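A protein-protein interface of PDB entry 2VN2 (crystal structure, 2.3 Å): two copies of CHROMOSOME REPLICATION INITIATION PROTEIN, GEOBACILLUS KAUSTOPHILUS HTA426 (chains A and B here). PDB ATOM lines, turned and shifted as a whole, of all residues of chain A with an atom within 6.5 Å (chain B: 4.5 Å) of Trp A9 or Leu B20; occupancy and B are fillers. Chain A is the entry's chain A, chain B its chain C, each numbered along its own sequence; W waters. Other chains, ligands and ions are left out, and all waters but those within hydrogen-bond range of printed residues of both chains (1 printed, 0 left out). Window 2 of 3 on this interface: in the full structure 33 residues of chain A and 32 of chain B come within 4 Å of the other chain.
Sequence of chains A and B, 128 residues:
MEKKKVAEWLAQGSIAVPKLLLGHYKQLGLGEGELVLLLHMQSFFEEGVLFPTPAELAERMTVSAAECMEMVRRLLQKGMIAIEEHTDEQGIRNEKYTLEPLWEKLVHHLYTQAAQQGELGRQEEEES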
ATOM      1  N   GLU A   2       4.943   1.666   2.364  1.00  0.00           N
ATOM      2  CA  GLU A   2       4.058   2.865   2.541  1.00  0.00           C
ATOM      3  C   GLU A   2       4.553   4.037   3.421  1.00  0.00           C
ATOM      4  O   GLU A   2       4.681   3.929   4.671  1.00  0.00           O
ATOM      5  CB  GLU A   2       2.662   2.475   2.974  1.00  0.00           C
ATOM      6  CG  GLU A   2       1.537   3.282   2.335  1.00  0.00           C
ATOM      7  CD  GLU A   2       0.985   4.369   3.254  1.00  0.00           C
ATOM      8  OE1 GLU A   2       0.711   3.989   4.415  1.00  0.00           O
ATOM      9  OE2 GLU A   2       0.800   5.565   2.814  1.00  0.00           O
ATOM     10  N   LYS A   4       3.300   7.006   4.729  1.00  0.00           N
ATOM     11  CA  LYS A   4       2.584   7.492   5.914  1.00  0.00           C
ATOM     12  C   LYS A   4       2.791   6.569   7.127  1.00  0.00           C
ATOM     13  O   LYS A   4       2.666   6.944   8.305  1.00  0.00           O
ATOM     14  CB  LYS A   4       1.093   7.582   5.572  1.00  0.00           C
ATOM     15  CG  LYS A   4       0.237   8.606   6.347  1.00  0.00           C
ATOM     16  CD  LYS A   4      -0.648   9.497   5.346  1.00  0.00           C
ATOM     17  CE  LYS A   4      -1.987   9.976   5.997  1.00  0.00           C
ATOM     18  NZ  LYS A   4      -1.855  10.021   7.555  1.00  0.00           N
ATOM     19  N   LYS A   5       3.122   5.339   6.818  1.00  0.00           N
ATOM     20  CA  LYS A   5       3.248   4.279   7.801  1.00  0.00           C
ATOM     21  C   LYS A   5       4.656   4.356   8.442  1.00  0.00           C
ATOM     22  O   LYS A   5       4.814   4.272   9.653  1.00  0.00           O
ATOM     23  CB  LYS A   5       3.030   2.899   7.080  1.00  0.00           C
ATOM     24  CG  LYS A   5       2.700   1.822   7.974  1.00  0.00           C
ATOM     25  CD  LYS A   5       1.475   2.145   8.748  1.00  0.00           C
ATOM     26  CE  LYS A   5       1.787   1.832  10.195  1.00  0.00           C
ATOM     27  NZ  LYS A   5       0.532   1.258  10.750  1.00  0.00           N
ATOM     28  N   VAL A   6       5.627   4.503   7.577  1.00  0.00           N
ATOM     29  CA  VAL A   6       6.991   4.672   7.975  1.00  0.00           C
ATOM     30  C   VAL A   6       7.140   5.835   8.878  1.00  0.00           C
ATOM     31  O   VAL A   6       7.766   5.678   9.930  1.00  0.00           O
ATOM     32  CB  VAL A   6       7.897   4.845   6.821  1.00  0.00           C
ATOM     33  CG1 VAL A   6       9.238   5.116   7.313  1.00  0.00           C
ATOM     34  CG2 VAL A   6       7.988   3.519   6.112  1.00  0.00           C
ATOM     35  N   ALA A   7       6.515   6.973   8.490  1.00  0.00           N
ATOM     36  CA  ALA A   7       6.475   8.212   9.254  1.00  0.00           C
ATOM     37  C   ALA A   7       5.867   7.947  10.616  1.00  0.00           C
ATOM     38  O   ALA A   7       6.447   8.400  11.635  1.00  0.00           O
ATOM     39  CB  ALA A   7       5.767   9.299   8.537  1.00  0.00           C
ATOM     40  N   GLU A   8       4.768   7.194  10.669  1.00  0.00           N
ATOM     41  CA  GLU A   8       4.156   6.831  11.978  1.00  0.00           C
ATOM     42  C   GLU A   8       5.075   5.923  12.779  1.00  0.00           C
ATOM     43  O   GLU A   8       5.191   6.130  13.954  1.00  0.00           O
ATOM     44  CB  GLU A   8       2.775   6.163  11.872  1.00  0.00           C
ATOM     45  CG  GLU A   8       2.403   5.393  13.214  1.00  0.00           C
ATOM     46  CD  GLU A   8       1.338   4.229  13.067  1.00  0.00           C
ATOM     47  OE1 GLU A   8       0.585   4.303  12.019  1.00  0.00           O
ATOM     48  OE2 GLU A   8       1.309   3.286  13.986  1.00  0.00           O
ATOM     49  N   TRP A   9       5.823   4.984  12.136  1.00  0.00           N
ATOM     50  CA  TRP A   9       6.826   4.324  12.900  1.00  0.00           C
ATOM     51  C   TRP A   9       7.880   5.268  13.466  1.00  0.00           C
ATOM     52  O   TRP A   9       8.163   5.173  14.673  1.00  0.00           O
ATOM     53  CB  TRP A   9       7.475   3.091  12.243  1.00  0.00           C
ATOM     54  CG  TRP A   9       6.471   2.083  11.833  1.00  0.00           C
ATOM     55  CD1 TRP A   9       5.270   1.844  12.402  1.00  0.00           C
ATOM     56  CD2 TRP A   9       6.555   1.276  10.674  1.00  0.00           C
ATOM     57  NE1 TRP A   9       4.589   0.888  11.685  1.00  0.00           N
ATOM     58  CE2 TRP A   9       5.375   0.515  10.609  1.00  0.00           C
ATOM     59  CE3 TRP A   9       7.548   1.063   9.712  1.00  0.00           C
ATOM     60  CZ2 TRP A   9       5.134  -0.400   9.553  1.00  0.00           C
ATOM     61  CZ3 TRP A   9       7.338   0.057   8.678  1.00  0.00           C
ATOM     62  CH2 TRP A   9       6.152  -0.613   8.613  1.00  0.00           C
ATOM     63  N   LEU A  10       8.453   6.132  12.609  1.00  0.00           N
ATOM     64  CA  LEU A  10       9.501   7.010  12.995  1.00  0.00           C
ATOM     65  C   LEU A  10       9.135   8.016  14.060  1.00  0.00           C
ATOM     66  O   LEU A  10      10.023   8.357  14.871  1.00  0.00           O
ATOM     67  CB  LEU A  10      10.109   7.722  11.811  1.00  0.00           C
ATOM     68  CG  LEU A  10      10.838   6.821  10.799  1.00  0.00           C
ATOM     69  CD1 LEU A  10      11.419   7.651   9.558  1.00  0.00           C
ATOM     70  CD2 LEU A  10      11.992   6.072  11.460  1.00  0.00           C
ATOM     71  N   ALA A  11       7.843   8.428  14.108  1.00  0.00           N
ATOM     72  CA  ALA A  11       7.275   9.352  15.108  1.00  0.00           C
ATOM     73  C   ALA A  11       7.027   8.758  16.467  1.00  0.00           C
ATOM     74  O   ALA A  11       6.782   9.488  17.431  1.00  0.00           O
ATOM     75  CB  ALA A  11       5.995   9.875  14.644  1.00  0.00           C
ATOM     76  N   GLN A  12       7.087   7.435  16.588  1.00  0.00           N
ATOM     77  CA  GLN A  12       6.902   6.793  17.909  1.00  0.00           C
ATOM     78  C   GLN A  12       7.957   7.234  18.933  1.00  0.00           C
ATOM     79  O   GLN A  12       7.694   7.272  20.116  1.00  0.00           O
ATOM     80  CB  GLN A  12       7.013   5.250  17.763  1.00  0.00           C
ATOM     81  CG  GLN A  12       6.050   4.739  16.794  1.00  0.00           C
ATOM     82  CD  GLN A  12       4.672   4.661  17.391  1.00  0.00           C
ATOM     83  OE1 GLN A  12       4.214   5.597  18.069  1.00  0.00           O
ATOM     84  NE2 GLN A  12       3.994   3.494  17.166  1.00  0.00           N
ATOM     85  N   GLY A  13       9.174   7.485  18.504  1.00  0.00           N
ATOM     86  CA  GLY A  13      10.106   7.865  19.522  1.00  0.00           C
ATOM     87  C   GLY A  13      10.802   6.792  20.333  1.00  0.00           C
ATOM     88  O   GLY A  13      10.754   5.617  20.026  1.00  0.00           O
ATOM     89  N   PRO B  18      14.322   2.722  21.040  1.00  0.00           N
ATOM     90  CA  PRO B  18      13.013   2.918  20.333  1.00  0.00           C
ATOM     91  C   PRO B  18      11.776   2.288  21.107  1.00  0.00           C
ATOM     92  O   PRO B  18      11.889   1.148  21.516  1.00  0.00           O
ATOM     93  CB  PRO B  18      13.279   2.261  18.961  1.00  0.00           C
ATOM     94  CG  PRO B  18      14.815   2.446  18.779  1.00  0.00           C
ATOM     95  CD  PRO B  18      15.371   2.222  20.108  1.00  0.00           C
ATOM     96  N   LYS B  19      10.691   3.060  21.317  1.00  0.00           N
ATOM     97  CA  LYS B  19       9.447   2.522  21.808  1.00  0.00           C
ATOM     98  C   LYS B  19       8.901   1.327  21.005  1.00  0.00           C
ATOM     99  O   LYS B  19       8.197   0.459  21.564  1.00  0.00           O
ATOM    100  CB  LYS B  19       8.382   3.638  21.880  1.00  0.00           C
ATOM    101  CG  LYS B  19       8.625   4.613  23.054  1.00  0.00           C
ATOM    102  CD  LYS B  19       7.634   5.684  23.197  1.00  0.00           C
ATOM    103  CE  LYS B  19       8.135   6.637  24.328  1.00  0.00           C
ATOM    104  NZ  LYS B  19       7.225   7.880  24.629  1.00  0.00           N
ATOM    105  N   LEU B  20       9.165   1.321  19.698  1.00  0.00           N
ATOM    106  CA  LEU B  20       8.866   0.196  18.813  1.00  0.00           C
ATOM    107  C   LEU B  20       9.632  -1.061  19.187  1.00  0.00           C
ATOM    108  O   LEU B  20       9.040  -2.124  19.091  1.00  0.00           O
ATOM    109  CB  LEU B  20       9.084   0.520  17.278  1.00  0.00           C
ATOM    110  CG  LEU B  20       8.106   1.440  16.521  1.00  0.00           C
ATOM    111  CD1 LEU B  20       8.404   1.483  15.007  1.00  0.00           C
ATOM    112  CD2 LEU B  20       6.705   1.026  16.725  1.00  0.00           C
ATOM    113  N   LEU B  21      10.941  -0.978  19.520  1.00  0.00           N
ATOM    114  CA  LEU B  21      11.603  -2.096  20.069  1.00  0.00           C
ATOM    115  C   LEU B  21      10.998  -2.503  21.429  1.00  0.00           C
ATOM    116  O   LEU B  21      10.628  -3.707  21.632  1.00  0.00           O
ATOM    117  CB  LEU B  21      13.116  -1.916  20.188  1.00  0.00           C
ATOM    118  CG  LEU B  21      14.015  -3.078  20.640  1.00  0.00           C
ATOM    119  CD1 LEU B  21      13.746  -4.358  19.742  1.00  0.00           C
ATOM    120  CD2 LEU B  21      15.483  -2.602  20.550  1.00  0.00           C
ATOM    121  N   LEU B  22      10.905  -1.580  22.380  1.00  0.00           N
ATOM    122  CA  LEU B  22      10.270  -1.923  23.689  1.00  0.00           C
ATOM    123  C   LEU B  22       8.928  -2.646  23.501  1.00  0.00           C
ATOM    124  O   LEU B  22       8.619  -3.620  24.181  1.00  0.00           O
ATOM    125  CB  LEU B  22       9.979  -0.656  24.408  1.00  0.00           C
ATOM    126  CG  LEU B  22       9.942  -0.714  25.911  1.00  0.00           C
ATOM    127  CD1 LEU B  22      11.080  -1.625  26.512  1.00  0.00           C
ATOM    128  CD2 LEU B  22       9.935   0.757  26.470  1.00  0.00           C
ATOM    129  N   GLY B  23       8.118  -2.161  22.561  1.00  0.00           N
ATOM    130  CA  GLY B  23       6.790  -2.700  22.307  1.00  0.00           C
ATOM    131  C   GLY B  23       6.738  -4.005  21.533  1.00  0.00           C
ATOM    132  O   GLY B  23       5.648  -4.614  21.443  1.00  0.00           O
ATOM    133  N   HIS B  24       7.858  -4.478  20.964  1.00  0.00           N
ATOM    134  CA  HIS B  24       7.727  -5.666  20.115  1.00  0.00           C
ATOM    135  C   HIS B  24       8.820  -6.683  20.249  1.00  0.00           C
ATOM    136  O   HIS B  24       8.788  -7.612  19.502  1.00  0.00           O
ATOM    137  CB  HIS B  24       7.610  -5.311  18.650  1.00  0.00           C
ATOM    138  CG  HIS B  24       6.499  -4.363  18.332  1.00  0.00           C
ATOM    139  ND1 HIS B  24       5.281  -4.791  17.854  1.00  0.00           N
ATOM    140  CD2 HIS B  24       6.415  -3.004  18.417  1.00  0.00           C
ATOM    141  CE1 HIS B  24       4.473  -3.746  17.694  1.00  0.00           C
ATOM    142  NE2 HIS B  24       5.154  -2.653  17.992  1.00  0.00           N
ATOM    143  N   LEU B 106      12.841  -6.207  12.992  1.00  0.00           N
ATOM    144  CA  LEU B 106      11.822  -5.340  13.591  1.00  0.00           C
ATOM    145  C   LEU B 106      10.974  -4.739  12.521  1.00  0.00           C
ATOM    146  O   LEU B 106       9.771  -4.791  12.644  1.00  0.00           O
ATOM    147  CB  LEU B 106      12.465  -4.235  14.489  1.00  0.00           C
ATOM    148  CG  LEU B 106      11.477  -3.267  15.037  1.00  0.00           C
ATOM    149  CD1 LEU B 106      10.169  -3.963  15.677  1.00  0.00           C
ATOM    150  CD2 LEU B 106      12.305  -2.421  16.066  1.00  0.00           C
ATOM    151  N   LEU B 110       6.995  -5.170  11.794  1.00  0.00           N
ATOM    152  CA  LEU B 110       5.993  -4.066  11.780  1.00  0.00           C
ATOM    153  C   LEU B 110       5.169  -3.975  10.480  1.00  0.00           C
ATOM    154  O   LEU B 110       4.000  -3.541  10.543  1.00  0.00           O
ATOM    155  CB  LEU B 110       6.634  -2.662  12.016  1.00  0.00           C
ATOM    156  CG  LEU B 110       7.436  -2.386  13.315  1.00  0.00           C
ATOM    157  CD1 LEU B 110       8.378  -1.094  13.092  1.00  0.00           C
ATOM    158  CD2 LEU B 110       6.487  -2.266  14.457  1.00  0.00           C
ATOM    159  N   TYR B 111       5.828  -4.219   9.336  1.00  0.00           N
ATOM    160  CA  TYR B 111       5.169  -4.329   7.992  1.00  0.00           C
ATOM    161  C   TYR B 111       4.117  -5.492   7.941  1.00  0.00           C
ATOM    162  O   TYR B 111       2.987  -5.270   7.558  1.00  0.00           O
ATOM    163  CB  TYR B 111       6.223  -4.575   6.847  1.00  0.00           C
ATOM    164  CG  TYR B 111       6.659  -3.335   6.133  1.00  0.00           C
ATOM    165  CD1 TYR B 111       8.000  -2.764   6.354  1.00  0.00           C
ATOM    166  CD2 TYR B 111       5.790  -2.661   5.258  1.00  0.00           C
ATOM    167  CE1 TYR B 111       8.489  -1.565   5.623  1.00  0.00           C
ATOM    168  CE2 TYR B 111       6.268  -1.416   4.611  1.00  0.00           C
ATOM    169  CZ  TYR B 111       7.641  -0.951   4.837  1.00  0.00           C
ATOM    170  OH  TYR B 111       8.054   0.146   4.249  1.00  0.00           O
ATOM    171  N   ALA B 114       1.266  -4.449  10.142  1.00  0.00           N
ATOM    172  CA  ALA B 114       0.434  -3.433   9.526  1.00  0.00           C
ATOM    173  C   ALA B 114      -0.456  -4.084   8.447  1.00  0.00           C
ATOM    174  O   ALA B 114      -1.612  -3.741   8.355  1.00  0.00           O
ATOM    175  CB  ALA B 114       1.210  -2.284   8.982  1.00  0.00           C
HETATM  176  O   HOH W   1       9.882   3.764  18.125  1.00  0.00           O
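The backbone NH (N) of Lys B19 sits at hydrogen-bond distance from the backbone carbonyl oxygen (O) of Gly A13 (2.9 Å).
N of Lys A4 sits close to OE2 of Glu A2 (3.5 Å).
Tyr B111 touches Glu A2. Val A6 touches Tyr B111 (CG2 to OH, 3.9 Å). Leu B20 touches Trp A9. Leu B110 touches Trp A9 (O to CZ2, 3.5 Å). Trp A9 touches Tyr B111 (CH2 to CD1, 3.6 Å). Gln A12 touches Lys B19. Gln A12 touches Leu B20 (NE2 to CD2, 3.7 Å). Gly A13 touches Pro B18 (O to CA, 3.5 Å).
Trp A9 touches just these residues of chain B: Leu B20, Leu B110 and Tyr B111. Leu B20 touches just these residues of chain A: Trp A9 (3.3 Å) and Gln A12 (3.7 Å). Printed residues of chain A within 4 Å of Tyr B111: Glu A2 (3.9 Å), Val A6 (3.9 Å) and Trp A9 (3.6 Å). Printed residues of chain B within 4 Å of Gln A12: Lys B19 (3.5 Å) and Leu B20 (3.7 Å). Of the printed residues of chain A, Leu B110 touches Trp A9. Printed residues of chain A within 4 Å of Pro B18: Gly A13 (3.5 Å).
Of the 11 printed residues of chain A, 5 touch a printed residue of chain B. Hydrophobic or aromatic side chains of chain A that line the printed part of chain B: Val A6 and Trp A9. Of the 11 printed residues of chain B, 5 touch a printed residue of chain A. Printed residues of chain B that touch a printed residue of chain A: Pro B18, Lys B19, Leu B20, Leu B110 and Tyr B111. Along chain B the printed residues that touch a printed residue of chain A span positions 18 to 111. Among the printed residues, 9 pairs touch across the chains.
No position is printed for both chains. Of the 9 pairs that touch across the chains among the printed residues, none has its exchanged pair printed and touching as well.
Water W1 lies within hydrogen-bond range of the backbone carbonyl oxygen (O) of Gly A13, the backbone NH (N) of Leu B20 and the backbone NH (N) of Lys B19.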
